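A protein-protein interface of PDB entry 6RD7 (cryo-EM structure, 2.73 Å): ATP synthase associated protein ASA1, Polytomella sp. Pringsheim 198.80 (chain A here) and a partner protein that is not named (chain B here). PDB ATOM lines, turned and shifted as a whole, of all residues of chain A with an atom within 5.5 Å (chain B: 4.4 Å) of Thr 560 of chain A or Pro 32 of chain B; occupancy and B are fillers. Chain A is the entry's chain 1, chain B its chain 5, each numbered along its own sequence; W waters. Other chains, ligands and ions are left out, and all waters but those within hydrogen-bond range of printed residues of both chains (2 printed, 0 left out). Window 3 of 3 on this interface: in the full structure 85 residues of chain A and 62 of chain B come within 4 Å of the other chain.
The backbone carbonyl oxygen of Glu 565 of chain A lies close to the side-chain sulfur of Met 35 of chain B, at 3.2 Å.
OD2 of Asp 557 of chain A is in salt-bridge range of NH1 of Arg 36 of chain B (2.6 Å).
The backbone carbonyl oxygen of Ile 556 of chain A lies within hydrogen-bond range of the side-chain hydroxyl of Thr 560 of chain A, 3.1 Å away.
The backbone carbonyl oxygen (O) of Glu 559 of chain A is in hydrogen-bond range of the backbone NH (N) of Glu 565 of chain A.
Among the printed residues, merely in contact across the chains: Ile 556 of chain A with Met 35 of chain B, Ile 556 of chain A with Arg 36 of chain B, Thr 560 of chain A with Pro 32 of chain B and Thr 560 of chain A with Met 35 of chain B.
Printed residues of chain B within 4 Å of Ile 556 of chain A: Met 35 (3.4 Å) and Arg 36 (3.7 Å).
Printed residues of chain B within 4 Å of Asp 557 of chain A: Arg 36.
Thr 560 of chain A touches two residues of chain B.
Thr 561 of chain A touches none of the printed residues of chain B.
Of the printed residues of chain B, Glu 565 of chain A touches Met 35 (3.2 Å).
Pro 32 of chain B touches just one residue of chain A: Thr 560.
Printed residues of chain A within 4 Å of Met 35 of chain B: Ile 556 (3.4 Å), Thr 560 (3.6 Å) and Glu 565 (3.2 Å).
Of the printed residues of chain A, Arg 36 of chain B touches Ile 556 and Asp 557.
The nearest printed residue of chain B that does not touch Glu 565 of chain A is Leu 31 of chain B (4.3 Å).
Of the 11 printed residues of chain B, 3 touch a printed residue of chain A.
Hydrophobic or aromatic side chains of chain B within 4 Å of the printed part of chain A: Pro 32 and Met 35.
Hydrophobic or aromatic side chains of chain A within 4 Å of the printed part of chain B: Ile 556.
Among the printed residues, Asp or Glu carboxylates within 4 Å of a Lys or Arg side-chain nitrogen of the other chain: Asp 557 of chain A with Arg 36 of chain B (2.6 Å).
Water W1 bridges the backbone carbonyl oxygen of Glu 565 of chain A and the side-chain sulfur of Met 35 of chain B.
Water W2 lies within hydrogen-bond range of OD1 of Asp 557 of chain A (2.8 Å), OG1 of Thr 560 of chain A (2.9 Å) and O of Pro 32 of chain B (3.0 Å).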
ATOM      1  N   LYS A 555     -12.866  15.073  28.028  1.00  0.00           N
ATOM      2  CA  LYS A 555     -13.571  14.846  26.768  1.00  0.00           C
ATOM      3  C   LYS A 555     -12.624  14.388  25.661  1.00  0.00           C
ATOM      4  O   LYS A 555     -12.977  13.512  24.859  1.00  0.00           O
ATOM      5  CB  LYS A 555     -14.304  16.112  26.353  1.00  0.00           C
ATOM      6  CG  LYS A 555     -15.466  16.454  27.242  1.00  0.00           C
ATOM      7  CD  LYS A 555     -15.865  17.890  27.063  1.00  0.00           C
ATOM      8  CE  LYS A 555     -16.816  18.314  28.138  1.00  0.00           C
ATOM      9  NZ  LYS A 555     -17.685  19.417  27.682  1.00  0.00           N
ATOM     10  N   ILE A 556     -11.418  14.958  25.605  1.00  0.00           N
ATOM     11  CA  ILE A 556     -10.426  14.521  24.624  1.00  0.00           C
ATOM     12  C   ILE A 556      -9.976  13.094  24.923  1.00  0.00           C
ATOM     13  O   ILE A 556      -9.767  12.282  24.010  1.00  0.00           O
ATOM     14  CB  ILE A 556      -9.246  15.513  24.598  1.00  0.00           C
ATOM     15  CG1 ILE A 556      -9.702  16.861  24.055  1.00  0.00           C
ATOM     16  CG2 ILE A 556      -8.118  15.024  23.729  1.00  0.00           C
ATOM     17  CD1 ILE A 556      -8.760  17.974  24.377  1.00  0.00           C
ATOM     18  N   ASP A 557      -9.879  12.747  26.206  1.00  0.00           N
ATOM     19  CA  ASP A 557      -9.537  11.386  26.588  1.00  0.00           C
ATOM     20  C   ASP A 557     -10.667  10.421  26.268  1.00  0.00           C
ATOM     21  O   ASP A 557     -10.416   9.250  25.970  1.00  0.00           O
ATOM     22  CB  ASP A 557      -9.194  11.333  28.074  1.00  0.00           C
ATOM     23  CG  ASP A 557      -7.808  11.858  28.371  1.00  0.00           C
ATOM     24  OD1 ASP A 557      -7.080  12.196  27.417  1.00  0.00           O
ATOM     25  OD2 ASP A 557      -7.446  11.940  29.560  1.00  0.00           O
ATOM     26  N   TRP A 558     -11.917  10.886  26.336  1.00  0.00           N
ATOM     27  CA  TRP A 558     -13.031  10.059  25.880  1.00  0.00           C
ATOM     28  C   TRP A 558     -12.940   9.801  24.389  1.00  0.00           C
ATOM     29  O   TRP A 558     -13.254   8.701  23.925  1.00  0.00           O
ATOM     30  CB  TRP A 558     -14.374  10.714  26.207  1.00  0.00           C
ATOM     31  CG  TRP A 558     -15.554   9.837  25.854  1.00  0.00           C
ATOM     32  CD1 TRP A 558     -16.178   8.954  26.674  1.00  0.00           C
ATOM     33  CD2 TRP A 558     -16.231   9.751  24.588  1.00  0.00           C
ATOM     34  NE1 TRP A 558     -17.198   8.327  26.009  1.00  0.00           N
ATOM     35  CE2 TRP A 558     -17.250   8.799  24.726  1.00  0.00           C
ATOM     36  CE3 TRP A 558     -16.068  10.385  23.353  1.00  0.00           C
ATOM     37  CZ2 TRP A 558     -18.100   8.465  23.685  1.00  0.00           C
ATOM     38  CZ3 TRP A 558     -16.912  10.054  22.324  1.00  0.00           C
ATOM     39  CH2 TRP A 558     -17.917   9.106  22.493  1.00  0.00           C
ATOM     40  N   GLU A 559     -12.563  10.824  23.620  1.00  0.00           N
ATOM     41  CA  GLU A 559     -12.412  10.659  22.177  1.00  0.00           C
ATOM     42  C   GLU A 559     -11.305   9.673  21.839  1.00  0.00           C
ATOM     43  O   GLU A 559     -11.459   8.846  20.936  1.00  0.00           O
ATOM     44  CB  GLU A 559     -12.122  12.002  21.522  1.00  0.00           C
ATOM     45  CG  GLU A 559     -13.322  12.668  20.931  1.00  0.00           C
ATOM     46  CD  GLU A 559     -12.990  14.006  20.322  1.00  0.00           C
ATOM     47  OE1 GLU A 559     -12.811  14.072  19.091  1.00  0.00           O
ATOM     48  OE2 GLU A 559     -12.895  14.994  21.073  1.00  0.00           O
ATOM     49  N   THR A 560     -10.181   9.751  22.549  1.00  0.00           N
ATOM     50  CA  THR A 560      -9.082   8.821  22.308  1.00  0.00           C
ATOM     51  C   THR A 560      -9.447   7.409  22.753  1.00  0.00           C
ATOM     52  O   THR A 560      -9.087   6.430  22.091  1.00  0.00           O
ATOM     53  CB  THR A 560      -7.824   9.315  23.022  1.00  0.00           C
ATOM     54  OG1 THR A 560      -7.537  10.652  22.605  1.00  0.00           O
ATOM     55  CG2 THR A 560      -6.627   8.445  22.705  1.00  0.00           C
ATOM     56  N   THR A 561     -10.196   7.289  23.850  1.00  0.00           N
ATOM     57  CA  THR A 561     -10.567   5.979  24.375  1.00  0.00           C
ATOM     58  C   THR A 561     -11.559   5.269  23.465  1.00  0.00           C
ATOM     59  O   THR A 561     -11.501   4.046  23.305  1.00  0.00           O
ATOM     60  CB  THR A 561     -11.154   6.133  25.777  1.00  0.00           C
ATOM     61  OG1 THR A 561     -10.355   7.047  26.531  1.00  0.00           O
ATOM     62  CG2 THR A 561     -11.177   4.816  26.499  1.00  0.00           C
ATOM     63  N   ASN A 562     -12.467   6.018  22.849  1.00  0.00           N
ATOM     64  CA  ASN A 562     -13.531   5.440  22.044  1.00  0.00           C
ATOM     65  C   ASN A 562     -13.191   5.391  20.566  1.00  0.00           C
ATOM     66  O   ASN A 562     -14.110   5.392  19.739  1.00  0.00           O
ATOM     67  CB  ASN A 562     -14.828   6.214  22.264  1.00  0.00           C
ATOM     68  CG  ASN A 562     -15.449   5.914  23.600  1.00  0.00           C
ATOM     69  OD1 ASN A 562     -15.046   6.461  24.618  1.00  0.00           O
ATOM     70  ND2 ASN A 562     -16.427   5.025  23.608  1.00  0.00           N
ATOM     71  N   ALA A 563     -11.895   5.363  20.232  1.00  0.00           N
ATOM     72  CA  ALA A 563     -11.375   5.198  18.869  1.00  0.00           C
ATOM     73  C   ALA A 563     -11.863   6.295  17.930  1.00  0.00           C
ATOM     74  O   ALA A 563     -12.063   6.080  16.735  1.00  0.00           O
ATOM     75  CB  ALA A 563     -11.700   3.811  18.310  1.00  0.00           C
ATOM     76  N   LEU A 564     -12.058   7.486  18.481  1.00  0.00           N
ATOM     77  CA  LEU A 564     -12.462   8.656  17.718  1.00  0.00           C
ATOM     78  C   LEU A 564     -11.392   9.733  17.779  1.00  0.00           C
ATOM     79  O   LEU A 564     -11.705  10.920  17.837  1.00  0.00           O
ATOM     80  CB  LEU A 564     -13.791   9.207  18.225  1.00  0.00           C
ATOM     81  CG  LEU A 564     -15.025   8.350  17.986  1.00  0.00           C
ATOM     82  CD1 LEU A 564     -16.124   8.770  18.931  1.00  0.00           C
ATOM     83  CD2 LEU A 564     -15.476   8.474  16.550  1.00  0.00           C
ATOM     84  N   GLU A 565     -10.122   9.328  17.783  1.00  0.00           N
ATOM     85  CA  GLU A 565      -9.042  10.298  17.862  1.00  0.00           C
ATOM     86  C   GLU A 565      -8.899  11.103  16.578  1.00  0.00           C
ATOM     87  O   GLU A 565      -8.400  12.228  16.616  1.00  0.00           O
ATOM     88  CB  GLU A 565      -7.730   9.597  18.212  1.00  0.00           C
ATOM     89  CG  GLU A 565      -7.208   8.663  17.147  1.00  0.00           C
ATOM     90  CD  GLU A 565      -7.626   7.232  17.382  1.00  0.00           C
ATOM     91  OE1 GLU A 565      -8.407   6.988  18.320  1.00  0.00           O
ATOM     92  OE2 GLU A 565      -7.178   6.350  16.626  1.00  0.00           O
ATOM     93  N   LEU B  26       2.250   3.771  20.582  1.00  0.00           N
ATOM     94  CA  LEU B  26       1.568   4.817  19.842  1.00  0.00           C
ATOM     95  C   LEU B  26       0.173   5.049  20.394  1.00  0.00           C
ATOM     96  O   LEU B  26      -0.173   6.178  20.747  1.00  0.00           O
ATOM     97  CB  LEU B  26       1.512   4.451  18.364  1.00  0.00           C
ATOM     98  CG  LEU B  26       0.879   5.491  17.453  1.00  0.00           C
ATOM     99  CD1 LEU B  26       1.661   6.786  17.509  1.00  0.00           C
ATOM    100  CD2 LEU B  26       0.826   4.956  16.047  1.00  0.00           C
ATOM    101  N   ASP B  27      -0.624   3.985  20.527  1.00  0.00           N
ATOM    102  CA  ASP B  27      -2.016   4.097  20.945  1.00  0.00           C
ATOM    103  C   ASP B  27      -2.166   4.564  22.385  1.00  0.00           C
ATOM    104  O   ASP B  27      -3.167   5.194  22.732  1.00  0.00           O
ATOM    105  CB  ASP B  27      -2.709   2.750  20.797  1.00  0.00           C
ATOM    106  CG  ASP B  27      -3.445   2.613  19.501  1.00  0.00           C
ATOM    107  OD1 ASP B  27      -3.923   3.631  18.971  1.00  0.00           O
ATOM    108  OD2 ASP B  27      -3.559   1.474  19.018  1.00  0.00           O
ATOM    109  N   THR B  28      -1.196   4.254  23.232  1.00  0.00           N
ATOM    110  CA  THR B  28      -1.336   4.424  24.669  1.00  0.00           C
ATOM    111  C   THR B  28      -0.549   5.607  25.206  1.00  0.00           C
ATOM    112  O   THR B  28      -1.075   6.367  26.021  1.00  0.00           O
ATOM    113  CB  THR B  28      -0.903   3.125  25.363  1.00  0.00           C
ATOM    114  OG1 THR B  28      -1.838   2.093  25.045  1.00  0.00           O
ATOM    115  CG2 THR B  28      -0.868   3.268  26.850  1.00  0.00           C
ATOM    116  N   GLN B  29       0.675   5.818  24.737  1.00  0.00           N
ATOM    117  CA  GLN B  29       1.523   6.876  25.260  1.00  0.00           C
ATOM    118  C   GLN B  29       1.610   8.073  24.324  1.00  0.00           C
ATOM    119  O   GLN B  29       1.602   9.216  24.783  1.00  0.00           O
ATOM    120  CB  GLN B  29       2.919   6.321  25.548  1.00  0.00           C
ATOM    121  CG  GLN B  29       2.909   5.000  26.280  1.00  0.00           C
ATOM    122  CD  GLN B  29       2.504   5.137  27.726  1.00  0.00           C
ATOM    123  OE1 GLN B  29       1.919   4.229  28.306  1.00  0.00           O
ATOM    124  NE2 GLN B  29       2.825   6.274  28.324  1.00  0.00           N
ATOM    125  N   LEU B  30       1.689   7.846  23.015  1.00  0.00           N
ATOM    126  CA  LEU B  30       1.934   8.955  22.106  1.00  0.00           C
ATOM    127  C   LEU B  30       0.636   9.603  21.645  1.00  0.00           C
ATOM    128  O   LEU B  30       0.516  10.832  21.672  1.00  0.00           O
ATOM    129  CB  LEU B  30       2.761   8.479  20.917  1.00  0.00           C
ATOM    130  CG  LEU B  30       4.107   7.893  21.340  1.00  0.00           C
ATOM    131  CD1 LEU B  30       4.705   7.037  20.247  1.00  0.00           C
ATOM    132  CD2 LEU B  30       5.065   8.991  21.749  1.00  0.00           C
ATOM    133  N   LEU B  31      -0.347   8.797  21.224  1.00  0.00           N
ATOM    134  CA  LEU B  31      -1.589   9.367  20.699  1.00  0.00           C
ATOM    135  C   LEU B  31      -2.440  10.105  21.729  1.00  0.00           C
ATOM    136  O   LEU B  31      -3.058  11.108  21.346  1.00  0.00           O
ATOM    137  CB  LEU B  31      -2.416   8.294  19.986  1.00  0.00           C
ATOM    138  CG  LEU B  31      -2.215   8.152  18.481  1.00  0.00           C
ATOM    139  CD1 LEU B  31      -3.168   7.118  17.922  1.00  0.00           C
ATOM    140  CD2 LEU B  31      -2.414   9.480  17.797  1.00  0.00           C
ATOM    141  N   PRO B  32      -2.560   9.675  23.030  1.00  0.00           N
ATOM    142  CA  PRO B  32      -3.269  10.539  23.986  1.00  0.00           C
ATOM    143  C   PRO B  32      -2.641  11.907  24.199  1.00  0.00           C
ATOM    144  O   PRO B  32      -3.358  12.907  24.262  1.00  0.00           O
ATOM    145  CB  PRO B  32      -3.242   9.711  25.271  1.00  0.00           C
ATOM    146  CG  PRO B  32      -3.341   8.365  24.789  1.00  0.00           C
ATOM    147  CD  PRO B  32      -2.437   8.321  23.606  1.00  0.00           C
ATOM    148  N   THR B  33      -1.311  11.962  24.267  1.00  0.00           N
ATOM    149  CA  THR B  33      -0.607  13.234  24.405  1.00  0.00           C
ATOM    150  C   THR B  33      -0.795  14.109  23.169  1.00  0.00           C
ATOM    151  O   THR B  33      -1.113  15.306  23.277  1.00  0.00           O
ATOM    152  CB  THR B  33       0.874  12.956  24.655  1.00  0.00           C
ATOM    153  OG1 THR B  33       1.050  12.450  25.981  1.00  0.00           O
ATOM    154  CG2 THR B  33       1.704  14.198  24.481  1.00  0.00           C
ATOM    155  N   ILE B  34      -0.616  13.510  21.988  1.00  0.00           N
ATOM    156  CA  ILE B  34      -0.781  14.210  20.718  1.00  0.00           C
ATOM    157  C   ILE B  34      -2.208  14.714  20.563  1.00  0.00           C
ATOM    158  O   ILE B  34      -2.430  15.843  20.122  1.00  0.00           O
ATOM    159  CB  ILE B  34      -0.371  13.285  19.556  1.00  0.00           C
ATOM    160  CG1 ILE B  34       1.141  13.177  19.474  1.00  0.00           C
ATOM    161  CG2 ILE B  34      -0.844  13.806  18.233  1.00  0.00           C
ATOM    162  CD1 ILE B  34       1.589  12.006  18.686  1.00  0.00           C
ATOM    163  N   MET B  35      -3.194  13.921  20.986  1.00  0.00           N
ATOM    164  CA  MET B  35      -4.581  14.332  20.819  1.00  0.00           C
ATOM    165  C   MET B  35      -4.989  15.382  21.834  1.00  0.00           C
ATOM    166  O   MET B  35      -5.819  16.234  21.524  1.00  0.00           O
ATOM    167  CB  MET B  35      -5.526  13.138  20.901  1.00  0.00           C
ATOM    168  CG  MET B  35      -5.553  12.269  19.676  1.00  0.00           C
ATOM    169  SD  MET B  35      -5.853  13.242  18.199  1.00  0.00           S
ATOM    170  CE  MET B  35      -4.321  13.014  17.310  1.00  0.00           C
ATOM    171  N   ARG B  36      -4.419  15.351  23.045  1.00  0.00           N
ATOM    172  CA  ARG B  36      -4.656  16.436  23.994  1.00  0.00           C
ATOM    173  C   ARG B  36      -4.133  17.754  23.451  1.00  0.00           C
ATOM    174  O   ARG B  36      -4.877  18.745  23.365  1.00  0.00           O
ATOM    175  CB  ARG B  36      -3.993  16.121  25.331  1.00  0.00           C
ATOM    176  CG  ARG B  36      -4.765  15.170  26.203  1.00  0.00           C
ATOM    177  CD  ARG B  36      -3.916  14.703  27.356  1.00  0.00           C
ATOM    178  NE  ARG B  36      -4.596  13.682  28.140  1.00  0.00           N
ATOM    179  CZ  ARG B  36      -4.315  13.404  29.406  1.00  0.00           C
ATOM    180  NH1 ARG B  36      -4.988  12.458  30.037  1.00  0.00           N
ATOM    181  NH2 ARG B  36      -3.367  14.075  30.039  1.00  0.00           N
HETATM  182  O   HOH W   1      -7.469  14.418  15.121  1.00  0.00           O
HETATM  183  O   HOH W   2      -6.203  11.985  24.753  1.00  0.00           O
